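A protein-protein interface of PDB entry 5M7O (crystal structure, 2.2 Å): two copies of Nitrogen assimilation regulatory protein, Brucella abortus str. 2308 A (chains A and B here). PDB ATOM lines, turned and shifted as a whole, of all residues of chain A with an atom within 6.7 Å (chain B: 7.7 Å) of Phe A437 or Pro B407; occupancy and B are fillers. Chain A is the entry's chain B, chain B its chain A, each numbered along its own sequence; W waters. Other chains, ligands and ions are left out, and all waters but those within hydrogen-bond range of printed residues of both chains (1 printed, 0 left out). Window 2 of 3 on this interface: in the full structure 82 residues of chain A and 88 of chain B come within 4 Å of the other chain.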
ATOM      1  N   TYR A 419       0.816  27.937   9.358  1.00  0.00           N
ATOM      2  CA  TYR A 419      -0.077  27.833  10.520  1.00  0.00           C
ATOM      3  C   TYR A 419      -0.149  26.374  10.961  1.00  0.00           C
ATOM      4  O   TYR A 419      -0.016  26.079  12.153  1.00  0.00           O
ATOM      5  CB  TYR A 419      -1.461  28.378  10.188  1.00  0.00           C
ATOM      6  CG  TYR A 419      -2.545  27.959  11.154  1.00  0.00           C
ATOM      7  CD1 TYR A 419      -3.226  26.746  10.989  1.00  0.00           C
ATOM      8  CD2 TYR A 419      -2.911  28.779  12.203  1.00  0.00           C
ATOM      9  CE1 TYR A 419      -4.195  26.353  11.865  1.00  0.00           C
ATOM     10  CE2 TYR A 419      -3.902  28.410  13.066  1.00  0.00           C
ATOM     11  CZ  TYR A 419      -4.535  27.190  12.892  1.00  0.00           C
ATOM     12  OH  TYR A 419      -5.525  26.825  13.768  1.00  0.00           O
ATOM     13  N   GLN A 423       1.150  24.823  14.534  1.00  0.00           N
ATOM     14  CA  GLN A 423       0.233  24.063  15.393  1.00  0.00           C
ATOM     15  C   GLN A 423       0.754  22.652  15.631  1.00  0.00           C
ATOM     16  O   GLN A 423       0.725  22.174  16.766  1.00  0.00           O
ATOM     17  CB  GLN A 423      -1.176  23.974  14.804  1.00  0.00           C
ATOM     18  CG  GLN A 423      -1.923  25.286  14.743  1.00  0.00           C
ATOM     19  CD  GLN A 423      -2.385  25.788  16.095  1.00  0.00           C
ATOM     20  OE1 GLN A 423      -1.990  25.271  17.122  1.00  0.00           O
ATOM     21  NE2 GLN A 423      -3.223  26.816  16.095  1.00  0.00           N
ATOM     22  N   ARG A 426       3.536  22.925  18.188  1.00  0.00           N
ATOM     23  CA  ARG A 426       2.829  23.224  19.469  1.00  0.00           C
ATOM     24  C   ARG A 426       2.163  22.030  20.129  1.00  0.00           C
ATOM     25  O   ARG A 426       2.108  21.975  21.353  1.00  0.00           O
ATOM     26  CB  ARG A 426       1.755  24.301  19.260  1.00  0.00           C
ATOM     27  CG  ARG A 426       0.953  24.768  20.492  1.00  0.00           C
ATOM     28  CD  ARG A 426      -0.512  24.908  20.109  1.00  0.00           C
ATOM     29  NE  ARG A 426      -1.399  25.395  21.161  1.00  0.00           N
ATOM     30  CZ  ARG A 426      -2.693  25.662  20.975  1.00  0.00           C
ATOM     31  NH1 ARG A 426      -3.245  25.483  19.779  1.00  0.00           N
ATOM     32  NH2 ARG A 426      -3.447  26.111  21.977  1.00  0.00           N
ATOM     33  N   PHE A 427       1.636  21.098  19.331  1.00  0.00           N
ATOM     34  CA  PHE A 427       1.119  19.806  19.856  1.00  0.00           C
ATOM     35  C   PHE A 427       2.146  18.652  19.884  1.00  0.00           C
ATOM     36  O   PHE A 427       1.769  17.508  20.128  1.00  0.00           O
ATOM     37  CB  PHE A 427      -0.181  19.402  19.129  1.00  0.00           C
ATOM     38  CG  PHE A 427      -1.352  20.217  19.550  1.00  0.00           C
ATOM     39  CD1 PHE A 427      -1.927  20.015  20.789  1.00  0.00           C
ATOM     40  CD2 PHE A 427      -1.853  21.226  18.732  1.00  0.00           C
ATOM     41  CE1 PHE A 427      -2.982  20.800  21.214  1.00  0.00           C
ATOM     42  CE2 PHE A 427      -2.916  22.011  19.150  1.00  0.00           C
ATOM     43  CZ  PHE A 427      -3.479  21.796  20.395  1.00  0.00           C
ATOM     44  N   SER A 432      -3.303  13.871  15.367  1.00  0.00           N
ATOM     45  CA  SER A 432      -4.723  13.721  15.744  1.00  0.00           C
ATOM     46  C   SER A 432      -5.198  14.848  16.669  1.00  0.00           C
ATOM     47  O   SER A 432      -6.339  15.300  16.534  1.00  0.00           O
ATOM     48  CB  SER A 432      -5.019  12.356  16.383  1.00  0.00           C
ATOM     49  OG  SER A 432      -4.570  12.297  17.724  1.00  0.00           O
ATOM     50  N   ARG A 433      -4.327  15.256  17.597  1.00  0.00           N
ATOM     51  CA  ARG A 433      -4.578  16.376  18.498  1.00  0.00           C
ATOM     52  C   ARG A 433      -4.581  17.690  17.744  1.00  0.00           C
ATOM     53  O   ARG A 433      -5.434  18.558  18.019  1.00  0.00           O
ATOM     54  CB  ARG A 433      -3.556  16.442  19.634  1.00  0.00           C
ATOM     55  CG  ARG A 433      -3.862  15.436  20.725  1.00  0.00           C
ATOM     56  CD  ARG A 433      -2.847  15.369  21.872  1.00  0.00           C
ATOM     57  NE  ARG A 433      -3.103  14.128  22.613  1.00  0.00           N
ATOM     58  CZ  ARG A 433      -2.357  13.614  23.591  1.00  0.00           C
ATOM     59  NH1 ARG A 433      -1.272  14.232  24.028  1.00  0.00           N
ATOM     60  NH2 ARG A 433      -2.716  12.450  24.145  1.00  0.00           N
ATOM     61  N   THR A 434      -3.651  17.826  16.794  1.00  0.00           N
ATOM     62  CA  THR A 434      -3.595  19.018  15.956  1.00  0.00           C
ATOM     63  C   THR A 434      -4.869  19.139  15.116  1.00  0.00           C
ATOM     64  O   THR A 434      -5.516  20.209  15.118  1.00  0.00           O
ATOM     65  CB  THR A 434      -2.356  19.057  15.040  1.00  0.00           C
ATOM     66  OG1 THR A 434      -1.182  19.172  15.845  1.00  0.00           O
ATOM     67  CG2 THR A 434      -2.402  20.271  14.151  1.00  0.00           C
ATOM     68  N   ALA A 435      -5.219  18.045  14.436  1.00  0.00           N
ATOM     69  CA  ALA A 435      -6.478  17.944  13.671  1.00  0.00           C
ATOM     70  C   ALA A 435      -7.662  18.487  14.467  1.00  0.00           C
ATOM     71  O   ALA A 435      -8.349  19.425  14.028  1.00  0.00           O
ATOM     72  CB  ALA A 435      -6.746  16.495  13.283  1.00  0.00           C
ATOM     73  N   GLU A 436      -7.842  17.942  15.667  1.00  0.00           N
ATOM     74  CA  GLU A 436      -9.008  18.267  16.481  1.00  0.00           C
ATOM     75  C   GLU A 436      -9.034  19.742  16.788  1.00  0.00           C
ATOM     76  O   GLU A 436     -10.079  20.383  16.661  1.00  0.00           O
ATOM     77  CB  GLU A 436      -9.072  17.469  17.786  1.00  0.00           C
ATOM     78  CG  GLU A 436     -10.519  17.159  18.208  1.00  0.00           C
ATOM     79  CD  GLU A 436     -10.663  16.769  19.684  1.00  0.00           C
ATOM     80  OE1 GLU A 436      -9.936  15.866  20.176  1.00  0.00           O
ATOM     81  OE2 GLU A 436     -11.517  17.378  20.363  1.00  0.00           O
ATOM     82  N   PHE A 437      -7.877  20.281  17.153  1.00  0.00           N
ATOM     83  CA  PHE A 437      -7.798  21.663  17.535  1.00  0.00           C
ATOM     84  C   PHE A 437      -8.007  22.557  16.320  1.00  0.00           C
ATOM     85  O   PHE A 437      -8.804  23.462  16.368  1.00  0.00           O
ATOM     86  CB  PHE A 437      -6.464  22.012  18.201  1.00  0.00           C
ATOM     87  CG  PHE A 437      -6.413  23.433  18.618  1.00  0.00           C
ATOM     88  CD1 PHE A 437      -6.052  24.413  17.705  1.00  0.00           C
ATOM     89  CD2 PHE A 437      -6.846  23.811  19.875  1.00  0.00           C
ATOM     90  CE1 PHE A 437      -6.080  25.750  18.052  1.00  0.00           C
ATOM     91  CE2 PHE A 437      -6.880  25.150  20.236  1.00  0.00           C
ATOM     92  CZ  PHE A 437      -6.505  26.121  19.320  1.00  0.00           C
ATOM     93  N   VAL A 438      -7.283  22.314  15.232  1.00  0.00           N
ATOM     94  CA  VAL A 438      -7.389  23.210  14.072  1.00  0.00           C
ATOM     95  C   VAL A 438      -8.743  23.130  13.362  1.00  0.00           C
ATOM     96  O   VAL A 438      -9.070  24.010  12.576  1.00  0.00           O
ATOM     97  CB  VAL A 438      -6.259  23.032  13.038  1.00  0.00           C
ATOM     98  CG1 VAL A 438      -4.912  23.303  13.679  1.00  0.00           C
ATOM     99  CG2 VAL A 438      -6.294  21.672  12.377  1.00  0.00           C
ATOM    100  N   GLY A 439      -9.515  22.075  13.614  1.00  0.00           N
ATOM    101  CA  GLY A 439     -10.861  21.945  13.055  1.00  0.00           C
ATOM    102  C   GLY A 439     -11.035  20.936  11.947  1.00  0.00           C
ATOM    103  O   GLY A 439     -12.057  20.940  11.286  1.00  0.00           O
ATOM    104  N   MET A 440     -10.071  20.030  11.771  1.00  0.00           N
ATOM    105  CA  MET A 440     -10.112  19.031  10.674  1.00  0.00           C
ATOM    106  C   MET A 440     -10.173  17.607  11.191  1.00  0.00           C
ATOM    107  O   MET A 440      -9.759  17.336  12.303  1.00  0.00           O
ATOM    108  CB  MET A 440      -8.888  19.167   9.769  1.00  0.00           C
ATOM    109  CG  MET A 440      -8.772  20.518   9.066  1.00  0.00           C
ATOM    110  SD  MET A 440      -7.286  20.535   8.042  1.00  0.00           S
ATOM    111  CE  MET A 440      -7.978  19.748   6.582  1.00  0.00           C
ATOM    112  N   GLN B 401       0.494  34.109  20.211  1.00  0.00           N
ATOM    113  CA  GLN B 401      -0.537  33.410  20.990  1.00  0.00           C
ATOM    114  C   GLN B 401      -1.939  33.526  20.404  1.00  0.00           C
ATOM    115  O   GLN B 401      -2.690  32.552  20.426  1.00  0.00           O
ATOM    116  CB  GLN B 401      -0.584  33.904  22.444  1.00  0.00           C
ATOM    117  CG  GLN B 401       0.640  33.571  23.299  1.00  0.00           C
ATOM    118  CD  GLN B 401       0.689  34.353  24.624  1.00  0.00           C
ATOM    119  OE1 GLN B 401      -0.345  34.730  25.181  1.00  0.00           O
ATOM    120  NE2 GLN B 401       1.895  34.595  25.129  1.00  0.00           N
ATOM    121  N   HIS B 402      -2.290  34.701  19.890  1.00  0.00           N
ATOM    122  CA  HIS B 402      -3.669  34.961  19.449  1.00  0.00           C
ATOM    123  C   HIS B 402      -4.039  34.291  18.120  1.00  0.00           C
ATOM    124  O   HIS B 402      -5.196  33.914  17.944  1.00  0.00           O
ATOM    125  CB  HIS B 402      -3.988  36.464  19.445  1.00  0.00           C
ATOM    126  CG  HIS B 402      -3.921  37.098  20.808  1.00  0.00           C
ATOM    127  ND1 HIS B 402      -3.032  38.107  21.123  1.00  0.00           N
ATOM    128  CD2 HIS B 402      -4.616  36.847  21.945  1.00  0.00           C
ATOM    129  CE1 HIS B 402      -3.188  38.457  22.388  1.00  0.00           C
ATOM    130  NE2 HIS B 402      -4.143  37.708  22.909  1.00  0.00           N
ATOM    131  N   ILE B 403      -3.084  34.125  17.202  1.00  0.00           N
ATOM    132  CA  ILE B 403      -3.324  33.277  16.017  1.00  0.00           C
ATOM    133  C   ILE B 403      -3.471  31.811  16.455  1.00  0.00           C
ATOM    134  O   ILE B 403      -4.420  31.128  16.070  1.00  0.00           O
ATOM    135  CB  ILE B 403      -2.218  33.372  14.926  1.00  0.00           C
ATOM    136  CG1 ILE B 403      -1.908  34.827  14.512  1.00  0.00           C
ATOM    137  CG2 ILE B 403      -2.615  32.563  13.693  1.00  0.00           C
ATOM    138  CD1 ILE B 403      -3.115  35.713  14.268  1.00  0.00           C
ATOM    139  N   MET B 404      -2.548  31.341  17.287  1.00  0.00           N
ATOM    140  CA  MET B 404      -2.512  29.934  17.700  1.00  0.00           C
ATOM    141  C   MET B 404      -3.739  29.481  18.502  1.00  0.00           C
ATOM    142  O   MET B 404      -4.008  28.284  18.594  1.00  0.00           O
ATOM    143  CB  MET B 404      -1.230  29.652  18.489  1.00  0.00           C
ATOM    144  CG  MET B 404       0.056  29.847  17.689  1.00  0.00           C
ATOM    145  SD  MET B 404       0.216  28.776  16.247  1.00  0.00           S
ATOM    146  CE  MET B 404       0.780  27.300  17.063  1.00  0.00           C
ATOM    147  N   ALA B 405      -4.475  30.433  19.068  1.00  0.00           N
ATOM    148  CA  ALA B 405      -5.725  30.149  19.771  1.00  0.00           C
ATOM    149  C   ALA B 405      -6.928  29.975  18.842  1.00  0.00           C
ATOM    150  O   ALA B 405      -7.965  29.488  19.279  1.00  0.00           O
ATOM    151  CB  ALA B 405      -6.000  31.260  20.769  1.00  0.00           C
ATOM    152  N   LEU B 406      -6.795  30.392  17.582  1.00  0.00           N
ATOM    153  CA  LEU B 406      -7.855  30.246  16.573  1.00  0.00           C
ATOM    154  C   LEU B 406      -7.745  28.967  15.745  1.00  0.00           C
ATOM    155  O   LEU B 406      -6.664  28.638  15.268  1.00  0.00           O
ATOM    156  CB  LEU B 406      -7.817  31.424  15.600  1.00  0.00           C
ATOM    157  CG  LEU B 406      -8.045  32.817  16.190  1.00  0.00           C
ATOM    158  CD1 LEU B 406      -7.810  33.847  15.102  1.00  0.00           C
ATOM    159  CD2 LEU B 406      -9.431  33.015  16.825  1.00  0.00           C
ATOM    160  N   PRO B 407      -8.878  28.271  15.510  1.00  0.00           N
ATOM    161  CA  PRO B 407      -8.821  27.165  14.541  1.00  0.00           C
ATOM    162  C   PRO B 407      -8.511  27.650  13.109  1.00  0.00           C
ATOM    163  O   PRO B 407      -8.390  28.846  12.864  1.00  0.00           O
ATOM    164  CB  PRO B 407     -10.208  26.532  14.622  1.00  0.00           C
ATOM    165  CG  PRO B 407     -10.864  27.132  15.822  1.00  0.00           C
ATOM    166  CD  PRO B 407     -10.243  28.478  16.013  1.00  0.00           C
ATOM    167  N   LEU B 408      -8.394  26.722  12.175  1.00  0.00           N
ATOM    168  CA  LEU B 408      -7.845  27.027  10.870  1.00  0.00           C
ATOM    169  C   LEU B 408      -8.693  28.040  10.084  1.00  0.00           C
ATOM    170  O   LEU B 408      -8.165  29.052   9.618  1.00  0.00           O
ATOM    171  CB  LEU B 408      -7.582  25.746  10.052  1.00  0.00           C
ATOM    172  CG  LEU B 408      -7.310  26.029   8.576  1.00  0.00           C
ATOM    173  CD1 LEU B 408      -5.970  26.737   8.405  1.00  0.00           C
ATOM    174  CD2 LEU B 408      -7.377  24.770   7.750  1.00  0.00           C
ATOM    175  N   ARG B 409      -9.980  27.771   9.922  1.00  0.00           N
ATOM    176  CA  ARG B 409     -10.816  28.644   9.113  1.00  0.00           C
ATOM    177  C   ARG B 409     -10.862  30.043   9.707  1.00  0.00           C
ATOM    178  O   ARG B 409     -10.811  31.018   8.980  1.00  0.00           O
ATOM    179  CB  ARG B 409     -12.247  28.132   9.017  1.00  0.00           C
ATOM    180  CG  ARG B 409     -13.159  29.037   8.167  1.00  0.00           C
ATOM    181  CD  ARG B 409     -14.530  28.428   7.868  1.00  0.00           C
ATOM    182  NE  ARG B 409     -15.357  28.354   9.084  1.00  0.00           N
ATOM    183  CZ  ARG B 409     -15.988  29.380   9.665  1.00  0.00           C
ATOM    184  NH1 ARG B 409     -15.921  30.605   9.153  1.00  0.00           N
ATOM    185  NH2 ARG B 409     -16.680  29.190  10.784  1.00  0.00           N
ATOM    186  N   GLU B 410     -10.984  30.138  11.025  1.00  0.00           N
ATOM    187  CA  GLU B 410     -11.060  31.446  11.662  1.00  0.00           C
ATOM    188  C   GLU B 410      -9.738  32.179  11.474  1.00  0.00           C
ATOM    189  O   GLU B 410      -9.725  33.379  11.192  1.00  0.00           O
ATOM    190  CB  GLU B 410     -11.474  31.358  13.146  1.00  0.00           C
ATOM    191  CG  GLU B 410     -12.950  30.997  13.354  1.00  0.00           C
ATOM    192  CD  GLU B 410     -13.241  29.490  13.381  1.00  0.00           C
ATOM    193  OE1 GLU B 410     -12.373  28.661  12.970  1.00  0.00           O
ATOM    194  OE2 GLU B 410     -14.367  29.137  13.848  1.00  0.00           O
ATOM    195  N   ALA B 411      -8.638  31.444  11.589  1.00  0.00           N
ATOM    196  CA  ALA B 411      -7.294  31.997  11.397  1.00  0.00           C
ATOM    197  C   ALA B 411      -7.131  32.477   9.964  1.00  0.00           C
ATOM    198  O   ALA B 411      -6.656  33.569   9.727  1.00  0.00           O
ATOM    199  CB  ALA B 411      -6.241  30.940  11.716  1.00  0.00           C
ATOM    200  N   ARG B 412      -7.572  31.659   9.021  1.00  0.00           N
ATOM    201  CA  ARG B 412      -7.452  31.976   7.611  1.00  0.00           C
ATOM    202  C   ARG B 412      -8.258  33.218   7.236  1.00  0.00           C
ATOM    203  O   ARG B 412      -7.761  34.094   6.534  1.00  0.00           O
ATOM    204  CB  ARG B 412      -7.910  30.784   6.804  1.00  0.00           C
ATOM    205  CG  ARG B 412      -7.790  30.955   5.316  1.00  0.00           C
ATOM    206  CD  ARG B 412      -8.065  29.620   4.676  1.00  0.00           C
ATOM    207  NE  ARG B 412      -9.461  29.197   4.848  1.00  0.00           N
ATOM    208  CZ  ARG B 412      -9.865  27.938   5.034  1.00  0.00           C
ATOM    209  NH1 ARG B 412      -8.997  26.932   5.117  1.00  0.00           N
ATOM    210  NH2 ARG B 412     -11.159  27.679   5.155  1.00  0.00           N
ATOM    211  N   GLU B 413      -9.493  33.304   7.719  1.00  0.00           N
ATOM    212  CA  GLU B 413     -10.358  34.452   7.413  1.00  0.00           C
ATOM    213  C   GLU B 413      -9.826  35.751   8.033  1.00  0.00           C
ATOM    214  O   GLU B 413      -9.940  36.817   7.433  1.00  0.00           O
ATOM    215  CB  GLU B 413     -11.803  34.209   7.864  1.00  0.00           C
ATOM    216  CG  GLU B 413     -12.503  33.121   7.056  1.00  0.00           C
ATOM    217  CD  GLU B 413     -13.934  32.817   7.502  1.00  0.00           C
ATOM    218  OE1 GLU B 413     -14.550  33.622   8.241  1.00  0.00           O
ATOM    219  OE2 GLU B 413     -14.445  31.753   7.078  1.00  0.00           O
HETATM  220  O   HOH W   1     -11.203  25.237  11.063  1.00  0.00           O
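The backbone carbonyl oxygen (O) of Met B404 sits at hydrogen-bond distance from the side-chain amide nitrogen (NE2) of Gln A423.
O of Met B404 is in hydrogen-bond range of NH1 of Arg A426, at 3.1 Å.
OH of Tyr A419 sits at hydrogen-bond distance from O of Leu B406.
OH of Tyr A419 sits at hydrogen-bond distance from N of Leu B408, 3.3 Å away.
The backbone NH (N) of Leu B408 lies within hydrogen-bond range of the backbone carbonyl oxygen (O) of Val A438 (2.8 Å).
The side-chain amide nitrogen (NE2) of Gln A423 sits at hydrogen-bond distance from the side-chain hydroxyl (OH) of Tyr A419 (3.3 Å).
The guanidinium group (NH1) of Arg A426 is in hydrogen-bond range of the side-chain amide oxygen (OE1) of Gln A423 (2.9 Å).
Among the printed residues, merely in contact across the chains: Tyr A419 with Pro B407 (3.2 Å), Tyr A419 with Ala B411 (3.7 Å), Gln A423 with Leu B406 (3.98 Å), Phe A437 with Met B404 (3.3 Å), Phe A437 with Ala B405 (3.7 Å), Phe A437 with Pro B407 (3.8 Å) and Val A438 with Pro B407 (3.4 Å).
Phe A437 touches just these residues of chain B: Met B404 (3.3 Å), Ala B405 (3.7 Å) and Pro B407 (3.8 Å).
Printed residues of chain A within 4 Å of Leu B406: Tyr A419 (2.6 Å) and Gln A423 (3.98 Å).
Of chain A, only Tyr A419, Phe A437 and Val A438 come within 4 Å of Pro B407.
Arg B409 touches none of the printed residues of chain A.
Of the printed residues of chain A, Ala B411 touches Tyr A419.
The nearest printed residue of chain B that does not touch Tyr A419 is Ile B403 (4.1 Å).
Of the 13 printed residues of chain A, 5 touch a printed residue of chain B.
Printed residues of chain A that touch a printed residue of chain B: Tyr A419, Gln A423, Arg A426, Phe A437 and Val A438.
Hydrophobic or aromatic side chains of chain A within 4 Å of the printed part of chain B: Tyr A419 and Phe A437.
Along chain A the printed residues that touch a printed residue of chain B span positions 419 to 438.
Among the printed residues, no Asp or Glu carboxylate lies within 4 Å of a Lys or Arg side-chain nitrogen of the other chain.
No position is printed for both chains.
Water W1 lies within hydrogen-bond range of O of Val A438 (2.9 Å), N of Arg B409 (3.0 Å) and N of Leu B408 (3.4 Å).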
